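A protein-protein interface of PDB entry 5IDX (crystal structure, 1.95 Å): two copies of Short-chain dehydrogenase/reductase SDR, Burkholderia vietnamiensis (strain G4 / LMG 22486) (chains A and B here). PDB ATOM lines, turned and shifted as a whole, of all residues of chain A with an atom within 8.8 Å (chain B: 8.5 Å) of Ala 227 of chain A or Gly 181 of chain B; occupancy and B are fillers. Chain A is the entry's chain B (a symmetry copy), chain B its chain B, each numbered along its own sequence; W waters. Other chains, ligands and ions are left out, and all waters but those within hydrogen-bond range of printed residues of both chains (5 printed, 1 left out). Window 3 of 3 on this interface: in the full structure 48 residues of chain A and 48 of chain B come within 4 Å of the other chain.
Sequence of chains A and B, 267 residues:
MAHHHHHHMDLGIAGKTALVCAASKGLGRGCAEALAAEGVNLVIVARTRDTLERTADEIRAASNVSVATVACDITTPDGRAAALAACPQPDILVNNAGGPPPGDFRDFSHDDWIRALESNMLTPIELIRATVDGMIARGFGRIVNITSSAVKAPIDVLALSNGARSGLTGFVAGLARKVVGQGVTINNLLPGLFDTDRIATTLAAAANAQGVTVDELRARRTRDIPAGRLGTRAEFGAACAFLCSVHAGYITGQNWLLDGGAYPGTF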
ATOM      1  N   LEU A 193     -32.325  13.191   7.749  1.00  0.00           N
ATOM      2  CA  LEU A 193     -32.116  13.341   6.314  1.00  0.00           C
ATOM      3  C   LEU A 193     -30.665  13.021   5.973  1.00  0.00           C
ATOM      4  O   LEU A 193     -29.747  13.667   6.488  1.00  0.00           O
ATOM      5  CB  LEU A 193     -32.472  14.754   5.850  1.00  0.00           C
ATOM      6  CG  LEU A 193     -32.450  14.956   4.331  1.00  0.00           C
ATOM      7  CD1 LEU A 193     -33.544  14.110   3.658  1.00  0.00           C
ATOM      8  CD2 LEU A 193     -32.614  16.428   3.987  1.00  0.00           C
ATOM      9  N   ARG A 221     -34.135  22.689   3.241  1.00  0.00           N
ATOM     10  CA  ARG A 221     -34.207  21.572   4.176  1.00  0.00           C
ATOM     11  C   ARG A 221     -33.016  21.550   5.125  1.00  0.00           C
ATOM     12  O   ARG A 221     -33.140  21.094   6.265  1.00  0.00           O
ATOM     13  CB  ARG A 221     -34.312  20.263   3.398  1.00  0.00           C
ATOM     14  CG  ARG A 221     -35.349  20.369   2.311  1.00  0.00           C
ATOM     15  CD  ARG A 221     -35.937  19.045   1.898  1.00  0.00           C
ATOM     16  NE  ARG A 221     -37.152  19.281   1.121  1.00  0.00           N
ATOM     17  CZ  ARG A 221     -37.674  18.425   0.249  1.00  0.00           C
ATOM     18  NH1 ARG A 221     -37.087  17.256   0.024  1.00  0.00           N
ATOM     19  NH2 ARG A 221     -38.780  18.745  -0.404  1.00  0.00           N
ATOM     20  N   THR A 222     -31.862  22.045   4.682  1.00  0.00           N
ATOM     21  CA  THR A 222     -30.725  22.134   5.588  1.00  0.00           C
ATOM     22  C   THR A 222     -30.968  23.172   6.680  1.00  0.00           C
ATOM     23  O   THR A 222     -30.502  23.000   7.815  1.00  0.00           O
ATOM     24  CB  THR A 222     -29.456  22.441   4.788  1.00  0.00           C
ATOM     25  OG1 THR A 222     -29.180  21.339   3.913  1.00  0.00           O
ATOM     26  CG2 THR A 222     -28.270  22.640   5.702  1.00  0.00           C
ATOM     27  N   ARG A 223     -31.727  24.228   6.377  1.00  0.00           N
ATOM     28  CA  ARG A 223     -32.056  25.212   7.401  1.00  0.00           C
ATOM     29  C   ARG A 223     -32.868  24.611   8.539  1.00  0.00           C
ATOM     30  O   ARG A 223     -32.846  25.150   9.649  1.00  0.00           O
ATOM     31  CB  ARG A 223     -32.815  26.397   6.796  1.00  0.00           C
ATOM     32  CG  ARG A 223     -31.929  27.380   6.045  1.00  0.00           C
ATOM     33  CD  ARG A 223     -32.673  28.668   5.713  1.00  0.00           C
ATOM     34  NE  ARG A 223     -33.840  28.446   4.862  1.00  0.00           N
ATOM     35  CZ  ARG A 223     -33.832  28.553   3.536  1.00  0.00           C
ATOM     36  NH1 ARG A 223     -32.712  28.877   2.900  1.00  0.00           N
ATOM     37  NH2 ARG A 223     -34.943  28.334   2.845  1.00  0.00           N
ATOM     38  N   ASP A 224     -33.575  23.509   8.301  1.00  0.00           N
ATOM     39  CA  ASP A 224     -34.321  22.862   9.370  1.00  0.00           C
ATOM     40  C   ASP A 224     -33.491  21.834  10.132  1.00  0.00           C
ATOM     41  O   ASP A 224     -34.032  21.146  11.004  1.00  0.00           O
ATOM     42  CB  ASP A 224     -35.585  22.202   8.810  1.00  0.00           C
ATOM     43  CG  ASP A 224     -36.663  23.217   8.447  1.00  0.00           C
ATOM     44  OD1 ASP A 224     -36.623  24.348   8.979  1.00  0.00           O
ATOM     45  OD2 ASP A 224     -37.554  22.882   7.635  1.00  0.00           O
ATOM     46  N   ILE A 225     -32.204  21.713   9.831  1.00  0.00           N
ATOM     47  CA  ILE A 225     -31.321  20.775  10.521  1.00  0.00           C
ATOM     48  C   ILE A 225     -30.299  21.592  11.306  1.00  0.00           C
ATOM     49  O   ILE A 225     -29.450  22.264  10.698  1.00  0.00           O
ATOM     50  CB  ILE A 225     -30.624  19.825   9.544  1.00  0.00           C
ATOM     51  CG1 ILE A 225     -31.649  19.095   8.675  1.00  0.00           C
ATOM     52  CG2 ILE A 225     -29.743  18.835  10.324  1.00  0.00           C
ATOM     53  CD1 ILE A 225     -31.023  18.350   7.504  1.00  0.00           C
ATOM     54  N   PRO A 226     -30.327  21.562  12.641  1.00  0.00           N
ATOM     55  CA  PRO A 226     -29.332  22.325  13.416  1.00  0.00           C
ATOM     56  C   PRO A 226     -27.883  21.989  13.069  1.00  0.00           C
ATOM     57  O   PRO A 226     -27.037  22.892  13.107  1.00  0.00           O
ATOM     58  CB  PRO A 226     -29.673  21.960  14.869  1.00  0.00           C
ATOM     59  CG  PRO A 226     -31.164  21.665  14.826  1.00  0.00           C
ATOM     60  CD  PRO A 226     -31.373  20.975  13.501  1.00  0.00           C
ATOM     61  N   ALA A 227     -27.569  20.731  12.724  1.00  0.00           N
ATOM     62  CA  ALA A 227     -26.204  20.407  12.310  1.00  0.00           C
ATOM     63  C   ALA A 227     -25.800  21.107  11.011  1.00  0.00           C
ATOM     64  O   ALA A 227     -24.603  21.185  10.714  1.00  0.00           O
ATOM     65  CB  ALA A 227     -26.029  18.899  12.157  1.00  0.00           C
ATOM     66  N   GLY A 228     -26.758  21.616  10.235  1.00  0.00           N
ATOM     67  CA  GLY A 228     -26.429  22.365   9.033  1.00  0.00           C
ATOM     68  C   GLY A 228     -25.882  21.548   7.880  1.00  0.00           C
ATOM     69  O   GLY A 228     -25.215  22.101   7.001  1.00  0.00           O
ATOM     70  N   ARG A 229     -26.146  20.250   7.854  1.00  0.00           N
ATOM     71  CA  ARG A 229     -25.682  19.373   6.786  1.00  0.00           C
ATOM     72  C   ARG A 229     -26.583  18.150   6.769  1.00  0.00           C
ATOM     73  O   ARG A 229     -27.377  17.937   7.685  1.00  0.00           O
ATOM     74  CB  ARG A 229     -24.228  18.941   6.992  1.00  0.00           C
ATOM     75  CG  ARG A 229     -23.993  18.127   8.275  1.00  0.00           C
ATOM     76  CD  ARG A 229     -22.584  17.533   8.262  1.00  0.00           C
ATOM     77  NE  ARG A 229     -22.217  16.757   9.452  1.00  0.00           N
ATOM     78  CZ  ARG A 229     -22.439  15.452   9.607  1.00  0.00           C
ATOM     79  NH1 ARG A 229     -23.069  14.758   8.664  1.00  0.00           N
ATOM     80  NH2 ARG A 229     -22.035  14.838  10.713  1.00  0.00           N
ATOM     81  N   LEU A 230     -26.443  17.340   5.721  1.00  0.00           N
ATOM     82  CA  LEU A 230     -27.087  16.033   5.691  1.00  0.00           C
ATOM     83  C   LEU A 230     -26.191  14.996   6.359  1.00  0.00           C
ATOM     84  O   LEU A 230     -24.974  15.179   6.478  1.00  0.00           O
ATOM     85  CB  LEU A 230     -27.387  15.597   4.255  1.00  0.00           C
ATOM     86  CG  LEU A 230     -28.180  16.525   3.329  1.00  0.00           C
ATOM     87  CD1 LEU A 230     -28.855  15.724   2.206  1.00  0.00           C
ATOM     88  CD2 LEU A 230     -29.187  17.365   4.089  1.00  0.00           C
ATOM     89  N   GLY A 231     -26.805  13.899   6.804  1.00  0.00           N
ATOM     90  CA  GLY A 231     -26.020  12.787   7.306  1.00  0.00           C
ATOM     91  C   GLY A 231     -25.352  12.010   6.186  1.00  0.00           C
ATOM     92  O   GLY A 231     -25.746  12.089   5.023  1.00  0.00           O
ATOM     93  N   GLU A 235     -21.300   7.566   8.495  1.00  0.00           N
ATOM     94  CA  GLU A 235     -21.488   7.720   9.935  1.00  0.00           C
ATOM     95  C   GLU A 235     -22.679   6.893  10.407  1.00  0.00           C
ATOM     96  O   GLU A 235     -22.681   6.387  11.536  1.00  0.00           O
ATOM     97  CB  GLU A 235     -21.643   9.202  10.316  1.00  0.00           C
ATOM     98  CG  GLU A 235     -22.939   9.852   9.853  1.00  0.00           C
ATOM     99  CD  GLU A 235     -22.893  11.363   9.947  1.00  0.00           C
ATOM    100  OE1 GLU A 235     -22.291  11.889  10.911  1.00  0.00           O
ATOM    101  OE2 GLU A 235     -23.448  12.022   9.044  1.00  0.00           O
ATOM    102  N   LEU A 258     -30.393   9.726  14.693  1.00  0.00           N
ATOM    103  CA  LEU A 258     -29.268  10.288  13.945  1.00  0.00           C
ATOM    104  C   LEU A 258     -29.853  11.312  12.984  1.00  0.00           C
ATOM    105  O   LEU A 258     -30.124  11.009  11.817  1.00  0.00           O
ATOM    106  CB  LEU A 258     -28.481   9.196  13.200  1.00  0.00           C
ATOM    107  CG  LEU A 258     -27.394   8.471  14.004  1.00  0.00           C
ATOM    108  CD1 LEU A 258     -27.994   7.691  15.151  1.00  0.00           C
ATOM    109  CD2 LEU A 258     -26.584   7.543  13.098  1.00  0.00           C
ATOM    110  N   ASP A 259     -30.067  12.535  13.488  1.00  0.00           N
ATOM    111  CA  ASP A 259     -30.783  13.515  12.679  1.00  0.00           C
ATOM    112  C   ASP A 259     -30.210  14.923  12.826  1.00  0.00           C
ATOM    113  O   ASP A 259     -30.897  15.894  12.495  1.00  0.00           O
ATOM    114  CB  ASP A 259     -32.287  13.518  13.036  1.00  0.00           C
ATOM    115  CG  ASP A 259     -32.584  14.187  14.386  1.00  0.00           C
ATOM    116  OD1 ASP A 259     -31.670  14.337  15.231  1.00  0.00           O
ATOM    117  OD2 ASP A 259     -33.755  14.556  14.612  1.00  0.00           O
ATOM    118  N   GLY A 260     -28.983  15.059  13.323  1.00  0.00           N
ATOM    119  CA  GLY A 260     -28.378  16.379  13.430  1.00  0.00           C
ATOM    120  C   GLY A 260     -29.111  17.330  14.352  1.00  0.00           C
ATOM    121  O   GLY A 260     -28.977  18.552  14.203  1.00  0.00           O
ATOM    122  N   GLY A 261     -29.864  16.805  15.320  1.00  0.00           N
ATOM    123  CA  GLY A 261     -30.617  17.648  16.240  1.00  0.00           C
ATOM    124  C   GLY A 261     -31.952  18.138  15.726  1.00  0.00           C
ATOM    125  O   GLY A 261     -32.583  18.979  16.387  1.00  0.00           O
ATOM    126  N   ALA A 262     -32.412  17.644  14.570  1.00  0.00           N
ATOM    127  CA  ALA A 262     -33.610  18.207  13.952  1.00  0.00           C
ATOM    128  C   ALA A 262     -34.839  18.055  14.850  1.00  0.00           C
ATOM    129  O   ALA A 262     -35.614  19.006  15.018  1.00  0.00           O
ATOM    130  CB  ALA A 262     -33.846  17.559  12.585  1.00  0.00           C
ATOM    131  N   ILE B 136     -16.057  25.599  19.901  1.00  0.00           N
ATOM    132  CA  ILE B 136     -16.652  26.251  18.739  1.00  0.00           C
ATOM    133  C   ILE B 136     -15.569  26.875  17.870  1.00  0.00           C
ATOM    134  O   ILE B 136     -15.591  26.743  16.642  1.00  0.00           O
ATOM    135  CB  ILE B 136     -17.695  27.293  19.184  1.00  0.00           C
ATOM    136  CG1 ILE B 136     -18.962  26.612  19.717  1.00  0.00           C
ATOM    137  CG2 ILE B 136     -18.016  28.273  18.046  1.00  0.00           C
ATOM    138  CD1 ILE B 136     -19.915  27.580  20.433  1.00  0.00           C
ATOM    139  N   GLY B 139     -14.015  24.349  15.816  1.00  0.00           N
ATOM    140  CA  GLY B 139     -14.894  23.585  14.953  1.00  0.00           C
ATOM    141  C   GLY B 139     -15.081  22.145  15.358  1.00  0.00           C
ATOM    142  O   GLY B 139     -15.543  21.341  14.543  1.00  0.00           O
ATOM    143  N   LEU B 175     -29.290  23.450  24.780  1.00  0.00           N
ATOM    144  CA  LEU B 175     -27.992  23.908  24.289  1.00  0.00           C
ATOM    145  C   LEU B 175     -27.503  23.064  23.119  1.00  0.00           C
ATOM    146  O   LEU B 175     -26.892  23.589  22.177  1.00  0.00           O
ATOM    147  CB  LEU B 175     -26.955  23.877  25.411  1.00  0.00           C
ATOM    148  CG  LEU B 175     -25.570  24.376  24.990  1.00  0.00           C
ATOM    149  CD1 LEU B 175     -25.668  25.821  24.501  1.00  0.00           C
ATOM    150  CD2 LEU B 175     -24.577  24.250  26.136  1.00  0.00           C
ATOM    151  N   ALA B 176     -27.761  21.756  23.160  1.00  0.00           N
ATOM    152  CA  ALA B 176     -27.205  20.861  22.153  1.00  0.00           C
ATOM    153  C   ALA B 176     -27.630  21.270  20.747  1.00  0.00           C
ATOM    154  O   ALA B 176     -26.836  21.191  19.806  1.00  0.00           O
ATOM    155  CB  ALA B 176     -27.623  19.423  22.450  1.00  0.00           C
ATOM    156  N   ARG B 177     -28.879  21.704  20.577  1.00  0.00           N
ATOM    157  CA  ARG B 177     -29.301  22.133  19.249  1.00  0.00           C
ATOM    158  C   ARG B 177     -28.644  23.440  18.832  1.00  0.00           C
ATOM    159  O   ARG B 177     -28.540  23.705  17.633  1.00  0.00           O
ATOM    160  CB  ARG B 177     -30.826  22.283  19.172  1.00  0.00           C
ATOM    161  CG  ARG B 177     -31.584  20.999  18.853  1.00  0.00           C
ATOM    162  CD  ARG B 177     -31.789  20.183  20.100  1.00  0.00           C
ATOM    163  NE  ARG B 177     -32.614  18.993  19.901  1.00  0.00           N
ATOM    164  CZ  ARG B 177     -32.857  18.109  20.866  1.00  0.00           C
ATOM    165  NH1 ARG B 177     -32.341  18.295  22.078  1.00  0.00           N
ATOM    166  NH2 ARG B 177     -33.606  17.042  20.630  1.00  0.00           N
ATOM    167  N   LYS B 178     -28.181  24.254  19.788  1.00  0.00           N
ATOM    168  CA  LYS B 178     -27.621  25.550  19.423  1.00  0.00           C
ATOM    169  C   LYS B 178     -26.192  25.448  18.900  1.00  0.00           C
ATOM    170  O   LYS B 178     -25.780  26.289  18.092  1.00  0.00           O
ATOM    171  CB  LYS B 178     -27.681  26.513  20.617  1.00  0.00           C
ATOM    172  N   VAL B 179     -25.422  24.439  19.318  1.00  0.00           N
ATOM    173  CA  VAL B 179     -23.994  24.392  19.004  1.00  0.00           C
ATOM    174  C   VAL B 179     -23.606  23.280  18.029  1.00  0.00           C
ATOM    175  O   VAL B 179     -22.445  23.258  17.578  1.00  0.00           O
ATOM    176  CB  VAL B 179     -23.137  24.296  20.287  1.00  0.00           C
ATOM    177  CG1 VAL B 179     -23.450  25.482  21.226  1.00  0.00           C
ATOM    178  CG2 VAL B 179     -23.349  22.968  20.999  1.00  0.00           C
ATOM    179  N   VAL B 180     -24.524  22.385  17.655  1.00  0.00           N
ATOM    180  CA  VAL B 180     -24.130  21.246  16.819  1.00  0.00           C
ATOM    181  C   VAL B 180     -23.694  21.708  15.427  1.00  0.00           C
ATOM    182  O   VAL B 180     -22.779  21.128  14.830  1.00  0.00           O
ATOM    183  CB  VAL B 180     -25.264  20.198  16.753  1.00  0.00           C
ATOM    184  CG1 VAL B 180     -26.582  20.809  16.227  1.00  0.00           C
ATOM    185  CG2 VAL B 180     -24.840  18.983  15.905  1.00  0.00           C
ATOM    186  N   GLY B 181     -24.331  22.747  14.885  1.00  0.00           N
ATOM    187  CA  GLY B 181     -23.916  23.292  13.601  1.00  0.00           C
ATOM    188  C   GLY B 181     -22.509  23.867  13.601  1.00  0.00           C
ATOM    189  O   GLY B 181     -21.954  24.116  12.523  1.00  0.00           O
ATOM    190  N   GLN B 182     -21.925  24.082  14.776  1.00  0.00           N
ATOM    191  CA  GLN B 182     -20.551  24.545  14.898  1.00  0.00           C
ATOM    192  C   GLN B 182     -19.593  23.402  15.227  1.00  0.00           C
ATOM    193  O   GLN B 182     -18.429  23.650  15.558  1.00  0.00           O
ATOM    194  CB  GLN B 182     -20.482  25.662  15.950  1.00  0.00           C
ATOM    195  CG  GLN B 182     -21.270  26.919  15.534  1.00  0.00           C
ATOM    196  CD  GLN B 182     -21.741  27.775  16.705  1.00  0.00           C
ATOM    197  OE1 GLN B 182     -22.570  27.350  17.510  1.00  0.00           O
ATOM    198  NE2 GLN B 182     -21.223  28.998  16.793  1.00  0.00           N
ATOM    199  N   GLY B 183     -20.056  22.157  15.137  1.00  0.00           N
ATOM    200  CA  GLY B 183     -19.189  21.008  15.304  1.00  0.00           C
ATOM    201  C   GLY B 183     -19.084  20.468  16.711  1.00  0.00           C
ATOM    202  O   GLY B 183     -18.234  19.611  16.962  1.00  0.00           O
ATOM    203  N   VAL B 184     -19.926  20.927  17.629  1.00  0.00           N
ATOM    204  CA  VAL B 184     -19.909  20.506  19.024  1.00  0.00           C
ATOM    205  C   VAL B 184     -21.170  19.700  19.286  1.00  0.00           C
ATOM    206  O   VAL B 184     -22.278  20.185  19.028  1.00  0.00           O
ATOM    207  CB  VAL B 184     -19.854  21.718  19.973  1.00  0.00           C
ATOM    208  CG1 VAL B 184     -19.807  21.257  21.431  1.00  0.00           C
ATOM    209  CG2 VAL B 184     -18.675  22.637  19.615  1.00  0.00           C
ATOM    210  N   THR B 185     -21.011  18.491  19.814  1.00  0.00           N
ATOM    211  CA  THR B 185     -22.154  17.704  20.262  1.00  0.00           C
ATOM    212  C   THR B 185     -22.164  17.602  21.783  1.00  0.00           C
ATOM    213  O   THR B 185     -21.122  17.683  22.443  1.00  0.00           O
ATOM    214  CB  THR B 185     -22.154  16.307  19.651  1.00  0.00           C
ATOM    215  OG1 THR B 185     -21.043  15.561  20.157  1.00  0.00           O
ATOM    216  CG2 THR B 185     -22.071  16.396  18.124  1.00  0.00           C
ATOM    217  N   GLY B 249     -20.824  13.031  14.787  1.00  0.00           N
ATOM    218  CA  GLY B 249     -21.109  14.459  14.695  1.00  0.00           C
ATOM    219  C   GLY B 249     -22.542  14.803  14.338  1.00  0.00           C
ATOM    220  O   GLY B 249     -22.923  15.975  14.448  1.00  0.00           O
ATOM    221  N   TYR B 250     -23.337  13.822  13.918  1.00  0.00           N
ATOM    222  CA  TYR B 250     -24.753  14.017  13.623  1.00  0.00           C
ATOM    223  C   TYR B 250     -25.636  13.602  14.792  1.00  0.00           C
ATOM    224  O   TYR B 250     -26.863  13.591  14.657  1.00  0.00           O
ATOM    225  CB  TYR B 250     -25.137  13.224  12.366  1.00  0.00           C
ATOM    226  CG  TYR B 250     -26.144  13.879  11.427  1.00  0.00           C
ATOM    227  CD1 TYR B 250     -25.961  15.188  10.961  1.00  0.00           C
ATOM    228  CD2 TYR B 250     -27.252  13.163  10.960  1.00  0.00           C
ATOM    229  CE1 TYR B 250     -26.869  15.773  10.077  1.00  0.00           C
ATOM    230  CE2 TYR B 250     -28.161  13.734  10.079  1.00  0.00           C
ATOM    231  CZ  TYR B 250     -27.962  15.036   9.640  1.00  0.00           C
ATOM    232  OH  TYR B 250     -28.856  15.590   8.760  1.00  0.00           O
ATOM    233  N   ILE B 251     -25.033  13.254  15.925  1.00  0.00           N
ATOM    234  CA  ILE B 251     -25.742  12.767  17.102  1.00  0.00           C
ATOM    235  C   ILE B 251     -25.577  13.810  18.195  1.00  0.00           C
ATOM    236  O   ILE B 251     -24.457  14.059  18.652  1.00  0.00           O
ATOM    237  CB  ILE B 251     -25.199  11.407  17.559  1.00  0.00           C
ATOM    238  CG1 ILE B 251     -25.321  10.377  16.433  1.00  0.00           C
ATOM    239  CG2 ILE B 251     -25.918  10.940  18.828  1.00  0.00           C
ATOM    240  CD1 ILE B 251     -24.693   9.026  16.792  1.00  0.00           C
ATOM    241  N   THR B 252     -26.678  14.422  18.620  1.00  0.00           N
ATOM    242  CA  THR B 252     -26.562  15.398  19.696  1.00  0.00           C
ATOM    243  C   THR B 252     -27.865  15.443  20.468  1.00  0.00           C
ATOM    244  O   THR B 252     -28.930  15.106  19.946  1.00  0.00           O
ATOM    245  CB  THR B 252     -26.191  16.786  19.177  1.00  0.00           C
ATOM    246  OG1 THR B 252     -25.739  17.601  20.272  1.00  0.00           O
ATOM    247  CG2 THR B 252     -27.400  17.444  18.496  1.00  0.00           C
HETATM  248  O   HOH W   1     -23.066  10.970  13.360  1.00  0.00           O
HETATM  249  O   HOH W   2     -32.629  15.541  17.644  1.00  0.00           O
HETATM  250  O   HOH W   3     -19.904  12.396  12.116  1.00  0.00           O
HETATM  251  O   HOH W   4     -31.618  15.210   9.751  1.00  0.00           O
HETATM  252  O   HOH W   5     -29.149  13.288  16.637  1.00  0.00           O
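N of Gly 181 of chain B sits close to O of Pro 226 of chain A (3.2 Å). The side-chain hydroxyl of Tyr 250 of chain B is in hydrogen-bond range of the backbone carbonyl oxygen of Leu 193 of chain A. The side-chain hydroxyl of Tyr 250 of chain B is in hydrogen-bond range of the backbone carbonyl oxygen of Arg 229 of chain A (3.0 Å). OH of Tyr 250 of chain B lies close to N of Gly 231 of chain A, 3.3 Å away. O of Tyr 250 of chain B sits at hydrogen-bond distance from N of Gly 260 of chain A (2.9 Å).
Arg 223 of chain A touches none of the printed residues of chain B. Printed residues of chain B within 4 Å of Ile 225 of chain A: Tyr 250 (3.7 Å). Of chain B, only Arg 177 (3.5 Å), Val 180 (3.6 Å) and Gly 181 (3.2 Å) come within 4 Å of Pro 226 of chain A. Of chain B, only Val 180, Gly 181 and Tyr 250 come within 4 Å of Ala 227 of chain A. Printed residues of chain B within 4 Å of Leu 230 of chain A: Tyr 250. Printed residues of chain B within 4 Å of Gly 260 of chain A: Val 180 and Tyr 250. Val 179 of chain B touches none of the printed residues of chain A. Of chain A, only Pro 226 (3.6 Å), Ala 227 (3.6 Å) and Gly 260 (3.9 Å) come within 4 Å of Val 180 of chain B. Gly 181 of chain B touches just these residues of chain A: Pro 226 and Ala 227. The nearest residue of chain B that does not touch Ala 227 of chain A is Gly 249 of chain B (4.8 Å). The nearest residue of chain A that does not touch Gly 181 of chain B is Gly 228 of chain A (4.7 Å).
No position is printed for both chains. Of the 20 pairs that touch across the chains among the printed residues, none has its exchanged pair printed and touching as well.
Of the 18 printed residues of chain A, 12 touch a printed residue of chain B. Along chain A the printed residues that touch a printed residue of chain B span positions 193 to 261. Among the printed residues, 20 pairs touch across the chains. Among the printed residues, no Asp or Glu carboxylate lies within 4 Å of a Lys or Arg side-chain nitrogen of the other chain.
Water W3 lies within hydrogen-bond range of the side-chain carboxylate of Glu 235 of chain A (2.7 Å) and the backbone NH of Gly 249 of chain B (2.9 Å). Water W1 lies within hydrogen-bond range of OE1 of Glu 235 of chain A (2.7 Å), N of Tyr 250 of chain B (2.9 Å) and N of Gly 249 of chain B (3.4 Å). Water W2 lies within hydrogen-bond range of OD1 of Asp 259 of chain A (2.9 Å) and NH2 of Arg 177 of chain B (3.5 Å). Water W4 lies within hydrogen-bond range of O of Asp 259 of chain A (2.9 Å), N of Leu 193 of chain A (2.9 Å) and OH of Tyr 250 of chain B (3.0 Å). Water W5 lies within hydrogen-bond range of the backbone carbonyl oxygen (O) of Tyr 250 of chain B, the side-chain carboxylate (OD1) of Asp 259 of chain A and the backbone NH (N) of Thr 252 of chain B.
The backbone carbonyl oxygen (O) of Leu 193 of chain A is in hydrogen-bond range of the backbone NH (N) of Gly 231 of chain A, 3.0 Å away. N of Ala 227 of chain A lies within hydrogen-bond range of O of Gly 260 of chain A (3.0 Å). NH1 of Arg 229 of chain A lies within salt-bridge range of OE2 of Glu 235 of chain A (2.8 Å). N of Gly 261 of chain A is in hydrogen-bond range of OD1 of Asp 259 of chain A. The side-chain carboxylate of Asp 259 of chain A sits at hydrogen-bond distance from the backbone NH of Ala 262 of chain A, 3.4 Å away.
Among the printed residues, pairs that only touch across the chains: Ile 225 of chain A with Tyr 250 of chain B (3.7 Å), Pro 226 of chain A with Arg 177 of chain B (3.5 Å), Pro 226 of chain A with Val 180 of chain B (3.6 Å), Ala 227 of chain A with Val 180 of chain B (3.6 Å), Ala 227 of chain A with Gly 181 of chain B (3.6 Å), Ala 227 of chain A with Tyr 250 of chain B (3.8 Å), Arg 229 of chain A with Gly 249 of chain B (3.7 Å), Leu 230 of chain A with Tyr 250 of chain B (3.6 Å), Glu 235 of chain A with Tyr 250 of chain B (3.5 Å), Leu 258 of chain A with Tyr 250 of chain B (3.7 Å), Leu 258 of chain A with Ile 251 of chain B (3.7 Å), Asp 259 of chain A with Tyr 250 of chain B (3.6 Å), Gly 260 of chain A with Val 180 of chain B (3.9 Å), Gly 261 of chain A with Arg 177 of chain B (3.3 Å) and Gly 261 of chain A with Thr 252 of chain B (3.9 Å).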
